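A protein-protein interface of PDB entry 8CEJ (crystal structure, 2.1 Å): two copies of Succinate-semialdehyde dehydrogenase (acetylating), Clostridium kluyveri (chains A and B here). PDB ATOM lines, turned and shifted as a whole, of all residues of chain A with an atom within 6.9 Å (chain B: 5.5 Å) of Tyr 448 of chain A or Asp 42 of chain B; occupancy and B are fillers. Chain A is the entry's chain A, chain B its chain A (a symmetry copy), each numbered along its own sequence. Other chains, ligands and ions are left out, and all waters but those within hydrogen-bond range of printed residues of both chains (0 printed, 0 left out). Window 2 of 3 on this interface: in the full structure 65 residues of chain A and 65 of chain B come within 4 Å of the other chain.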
ATOM      1  N   PRO A 446      -1.180  25.915   7.628  1.00  0.00           N
ATOM      2  CA  PRO A 446      -0.772  27.013   6.747  1.00  0.00           C
ATOM      3  C   PRO A 446      -1.368  26.868   5.355  1.00  0.00           C
ATOM      4  O   PRO A 446      -1.564  25.762   4.846  1.00  0.00           O
ATOM      5  CB  PRO A 446       0.757  26.894   6.712  1.00  0.00           C
ATOM      6  CG  PRO A 446       1.111  26.116   7.942  1.00  0.00           C
ATOM      7  CD  PRO A 446      -0.024  25.157   8.134  1.00  0.00           C
ATOM      8  N   SER A 447      -1.665  28.014   4.742  1.00  0.00           N
ATOM      9  CA  SER A 447      -2.207  28.057   3.395  1.00  0.00           C
ATOM     10  C   SER A 447      -1.069  28.166   2.381  1.00  0.00           C
ATOM     11  O   SER A 447       0.111  28.154   2.735  1.00  0.00           O
ATOM     12  CB  SER A 447      -3.186  29.221   3.248  1.00  0.00           C
ATOM     13  OG  SER A 447      -2.510  30.464   3.325  1.00  0.00           O
ATOM     14  N   TYR A 448      -1.431  28.288   1.101  1.00  0.00           N
ATOM     15  CA  TYR A 448      -0.422  28.324   0.044  1.00  0.00           C
ATOM     16  C   TYR A 448       0.547  29.482   0.246  1.00  0.00           C
ATOM     17  O   TYR A 448       1.768  29.305   0.167  1.00  0.00           O
ATOM     18  CB  TYR A 448      -1.092  28.415  -1.327  1.00  0.00           C
ATOM     19  CG  TYR A 448      -0.137  28.212  -2.486  1.00  0.00           C
ATOM     20  CD1 TYR A 448       0.594  29.272  -3.007  1.00  0.00           C
ATOM     21  CD2 TYR A 448       0.033  26.958  -3.057  1.00  0.00           C
ATOM     22  CE1 TYR A 448       1.469  29.089  -4.061  1.00  0.00           C
ATOM     23  CE2 TYR A 448       0.905  26.765  -4.112  1.00  0.00           C
ATOM     24  CZ  TYR A 448       1.621  27.833  -4.611  1.00  0.00           C
ATOM     25  OH  TYR A 448       2.489  27.645  -5.661  1.00  0.00           O
ATOM     26  N   GLU A 449       0.019  30.682   0.500  1.00  0.00           N
ATOM     27  CA  GLU A 449       0.891  31.816   0.777  1.00  0.00           C
ATOM     28  C   GLU A 449       1.652  31.626   2.081  1.00  0.00           C
ATOM     29  O   GLU A 449       2.794  32.079   2.204  1.00  0.00           O
ATOM     30  CB  GLU A 449       0.081  33.112   0.828  1.00  0.00           C
ATOM     31  CG  GLU A 449       0.937  34.364   0.937  1.00  0.00           C
ATOM     32  CD  GLU A 449       0.230  35.502   1.644  1.00  0.00           C
ATOM     33  OE1 GLU A 449      -0.642  35.226   2.494  1.00  0.00           O
ATOM     34  OE2 GLU A 449       0.550  36.674   1.351  1.00  0.00           O
ATOM     35  N   GLU A 450       1.039  30.960   3.061  1.00  0.00           N
ATOM     36  CA  GLU A 450       1.705  30.738   4.337  1.00  0.00           C
ATOM     37  C   GLU A 450       2.794  29.676   4.242  1.00  0.00           C
ATOM     38  O   GLU A 450       3.681  29.639   5.100  1.00  0.00           O
ATOM     39  CB  GLU A 450       0.673  30.358   5.401  1.00  0.00           C
ATOM     40  CG  GLU A 450      -0.308  31.480   5.719  1.00  0.00           C
ATOM     41  CD  GLU A 450      -1.438  31.041   6.625  1.00  0.00           C
ATOM     42  OE1 GLU A 450      -1.969  29.930   6.423  1.00  0.00           O
ATOM     43  OE2 GLU A 450      -1.795  31.811   7.541  1.00  0.00           O
ATOM     44  N   ILE A 451       2.758  28.832   3.214  1.00  0.00           N
ATOM     45  CA  ILE A 451       3.779  27.804   3.032  1.00  0.00           C
ATOM     46  C   ILE A 451       4.916  28.298   2.145  1.00  0.00           C
ATOM     47  O   ILE A 451       6.089  28.204   2.513  1.00  0.00           O
ATOM     48  CB  ILE A 451       3.143  26.516   2.463  1.00  0.00           C
ATOM     49  CG1 ILE A 451       2.138  25.925   3.453  1.00  0.00           C
ATOM     50  CG2 ILE A 451       4.220  25.492   2.134  1.00  0.00           C
ATOM     51  CD1 ILE A 451       1.281  24.823   2.864  1.00  0.00           C
ATOM     52  N   TRP A 452       4.589  28.837   0.968  1.00  0.00           N
ATOM     53  CA  TRP A 452       5.586  29.228  -0.021  1.00  0.00           C
ATOM     54  C   TRP A 452       5.742  30.742  -0.139  1.00  0.00           C
ATOM     55  O   TRP A 452       6.213  31.228  -1.172  1.00  0.00           O
ATOM     56  CB  TRP A 452       5.234  28.644  -1.391  1.00  0.00           C
ATOM     57  CG  TRP A 452       4.933  27.175  -1.391  1.00  0.00           C
ATOM     58  CD1 TRP A 452       3.708  26.591  -1.540  1.00  0.00           C
ATOM     59  CD2 TRP A 452       5.874  26.104  -1.247  1.00  0.00           C
ATOM     60  NE1 TRP A 452       3.828  25.224  -1.496  1.00  0.00           N
ATOM     61  CE2 TRP A 452       5.147  24.898  -1.316  1.00  0.00           C
ATOM     62  CE3 TRP A 452       7.259  26.046  -1.064  1.00  0.00           C
ATOM     63  CZ2 TRP A 452       5.758  23.650  -1.209  1.00  0.00           C
ATOM     64  CZ3 TRP A 452       7.863  24.806  -0.958  1.00  0.00           C
ATOM     65  CH2 TRP A 452       7.114  23.625  -1.029  1.00  0.00           C
ATOM     66  N   GLY A 453       5.360  31.492   0.890  1.00  0.00           N
ATOM     67  CA  GLY A 453       5.344  32.946   0.823  1.00  0.00           C
ATOM     68  C   GLY A 453       6.613  33.623   0.345  1.00  0.00           C
ATOM     69  O   GLY A 453       7.619  33.661   1.051  1.00  0.00           O
ATOM     70  OXT GLY A 453       6.657  34.158  -0.765  1.00  0.00           O
ATOM     71  N   GLY B  37      10.890  21.566  -3.385  1.00  0.00           N
ATOM     72  CA  GLY B  37       9.574  21.166  -2.921  1.00  0.00           C
ATOM     73  C   GLY B  37       8.443  21.881  -3.623  1.00  0.00           C
ATOM     74  O   GLY B  37       7.348  21.326  -3.759  1.00  0.00           O
ATOM     75  N   LYS B  38       8.680  23.110  -4.083  1.00  0.00           N
ATOM     76  CA  LYS B  38       7.618  23.867  -4.736  1.00  0.00           C
ATOM     77  C   LYS B  38       7.257  23.269  -6.089  1.00  0.00           C
ATOM     78  O   LYS B  38       6.079  23.233  -6.462  1.00  0.00           O
ATOM     79  CB  LYS B  38       8.031  25.331  -4.887  1.00  0.00           C
ATOM     80  CG  LYS B  38       6.980  26.201  -5.559  1.00  0.00           C
ATOM     81  CD  LYS B  38       7.425  27.648  -5.653  1.00  0.00           C
ATOM     82  CE  LYS B  38       6.460  28.463  -6.500  1.00  0.00           C
ATOM     83  NZ  LYS B  38       5.066  28.396  -5.984  1.00  0.00           N
ATOM     84  N   VAL B  39       8.254  22.789  -6.838  1.00  0.00           N
ATOM     85  CA  VAL B  39       7.972  22.245  -8.164  1.00  0.00           C
ATOM     86  C   VAL B  39       7.227  20.918  -8.057  1.00  0.00           C
ATOM     87  O   VAL B  39       6.459  20.557  -8.958  1.00  0.00           O
ATOM     88  CB  VAL B  39       9.274  22.111  -8.978  1.00  0.00           C
ATOM     89  CG1 VAL B  39      10.147  20.986  -8.437  1.00  0.00           C
ATOM     90  CG2 VAL B  39       8.964  21.905 -10.456  1.00  0.00           C
ATOM     91  N   VAL B  40       7.424  20.177  -6.964  1.00  0.00           N
ATOM     92  CA  VAL B  40       6.640  18.965  -6.749  1.00  0.00           C
ATOM     93  C   VAL B  40       5.227  19.322  -6.316  1.00  0.00           C
ATOM     94  O   VAL B  40       4.264  18.629  -6.667  1.00  0.00           O
ATOM     95  CB  VAL B  40       7.338  18.055  -5.721  1.00  0.00           C
ATOM     96  CG1 VAL B  40       6.500  16.815  -5.443  1.00  0.00           C
ATOM     97  CG2 VAL B  40       8.722  17.669  -6.214  1.00  0.00           C
ATOM     98  N   TYR B  41       5.075  20.408  -5.557  1.00  0.00           N
ATOM     99  CA  TYR B  41       3.746  20.879  -5.184  1.00  0.00           C
ATOM    100  C   TYR B  41       2.984  21.378  -6.406  1.00  0.00           C
ATOM    101  O   TYR B  41       1.803  21.061  -6.585  1.00  0.00           O
ATOM    102  CB  TYR B  41       3.865  21.984  -4.132  1.00  0.00           C
ATOM    103  CG  TYR B  41       2.569  22.330  -3.430  1.00  0.00           C
ATOM    104  CD1 TYR B  41       1.621  23.147  -4.035  1.00  0.00           C
ATOM    105  CD2 TYR B  41       2.302  21.855  -2.153  1.00  0.00           C
ATOM    106  CE1 TYR B  41       0.440  23.466  -3.396  1.00  0.00           C
ATOM    107  CE2 TYR B  41       1.124  22.172  -1.504  1.00  0.00           C
ATOM    108  CZ  TYR B  41       0.198  22.978  -2.130  1.00  0.00           C
ATOM    109  OH  TYR B  41      -0.977  23.297  -1.489  1.00  0.00           O
ATOM    110  N   ASP B  42       3.648  22.159  -7.265  1.00  0.00           N
ATOM    111  CA  ASP B  42       2.967  22.774  -8.398  1.00  0.00           C
ATOM    112  C   ASP B  42       2.674  21.785  -9.520  1.00  0.00           C
ATOM    113  O   ASP B  42       1.814  22.061 -10.362  1.00  0.00           O
ATOM    114  CB  ASP B  42       3.794  23.940  -8.940  1.00  0.00           C
ATOM    115  CG  ASP B  42       3.987  25.042  -7.918  1.00  0.00           C
ATOM    116  OD1 ASP B  42       3.227  25.083  -6.927  1.00  0.00           O
ATOM    117  OD2 ASP B  42       4.899  25.873  -8.109  1.00  0.00           O
ATOM    118  N   ASN B  43       3.364  20.645  -9.556  1.00  0.00           N
ATOM    119  CA  ASN B  43       3.143  19.624 -10.574  1.00  0.00           C
ATOM    120  C   ASN B  43       2.608  18.335  -9.962  1.00  0.00           C
ATOM    121  O   ASN B  43       2.901  17.242 -10.448  1.00  0.00           O
ATOM    122  CB  ASN B  43       4.428  19.353 -11.354  1.00  0.00           C
ATOM    123  CG  ASN B  43       4.897  20.558 -12.145  1.00  0.00           C
ATOM    124  OD1 ASN B  43       4.517  20.739 -13.302  1.00  0.00           O
ATOM    125  ND2 ASN B  43       5.727  21.388 -11.526  1.00  0.00           N
ATOM    126  N   ALA B  44       1.813  18.452  -8.896  1.00  0.00           N
ATOM    127  CA  ALA B  44       1.348  17.268  -8.182  1.00  0.00           C
ATOM    128  C   ALA B  44       0.363  16.458  -9.015  1.00  0.00           C
ATOM    129  O   ALA B  44       0.379  15.223  -8.974  1.00  0.00           O
ATOM    130  CB  ALA B  44       0.716  17.674  -6.851  1.00  0.00           C
ATOM    131  N   GLU B  45      -0.503  17.133  -9.777  1.00  0.00           N
ATOM    132  CA  GLU B  45      -1.496  16.417 -10.573  1.00  0.00           C
ATOM    133  C   GLU B  45      -0.837  15.586 -11.668  1.00  0.00           C
ATOM    134  O   GLU B  45      -1.281  14.470 -11.958  1.00  0.00           O
ATOM    135  CB  GLU B  45      -2.500  17.399 -11.179  1.00  0.00           C
ATOM    136  CG  GLU B  45      -3.538  17.929 -10.200  1.00  0.00           C
ATOM    137  CD  GLU B  45      -2.990  18.999  -9.278  1.00  0.00           C
ATOM    138  OE1 GLU B  45      -1.869  19.488  -9.528  1.00  0.00           O
ATOM    139  OE2 GLU B  45      -3.685  19.353  -8.302  1.00  0.00           O
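The side-chain hydroxyl (OH) of Tyr 448 of chain A sits at hydrogen-bond distance from the side-chain amino group (NZ) of Lys 38 of chain B, at 2.7 Å. OH of Tyr 448 of chain A is in hydrogen-bond range of OD1 of Asp 42 of chain B.
NZ of Lys 38 of chain B lies within salt-bridge range of OD2 of Asp 42 of chain B, at 3.3 Å.
Among the printed residues, pairs that only touch across the chains: Tyr 448 of chain A with Tyr 41 of chain B (3.4 Å), Trp 452 of chain A with Gly 37 of chain B (3.4 Å), Trp 452 of chain A with Lys 38 of chain B (3.5 Å) and Trp 452 of chain A with Tyr 41 of chain B (3.7 Å).
Of the printed residues of chain B, Tyr 448 of chain A touches Lys 38, Tyr 41 and Asp 42. Printed residues of chain B within 4 Å of Trp 452 of chain A: Gly 37, Lys 38 and Tyr 41. Printed residues of chain A within 4 Å of Gly 37 of chain B: Trp 452 (3.4 Å). Printed residues of chain A within 4 Å of Lys 38 of chain B: Tyr 448 (2.7 Å) and Trp 452 (3.5 Å). Val 39 of chain B touches none of the printed residues of chain A. Of the printed residues of chain A, Tyr 41 of chain B touches Tyr 448 (3.4 Å) and Trp 452 (3.7 Å). Asp 42 of chain B touches just one residue of chain A: Tyr 448 (3.0 Å).
Printed residues of chain A that touch a printed residue of chain B: Tyr 448 and Trp 452. Hydrophobic or aromatic side chains of chain A that line the printed part of chain B: Tyr 448 and Trp 452. Along chain A the printed residues that touch a printed residue of chain B span positions 448 to 452. Of the 9 printed residues of chain B, 4 touch a printed residue of chain A. Hydrophobic or aromatic side chains of chain B within 4 Å of the printed part of chain A: Tyr 41. Among the printed residues, 6 pairs touch across the chains.
No position is printed for both chains. Of the 6 pairs that touch across the chains among the printed residues, none has its exchanged pair printed and touching as well.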
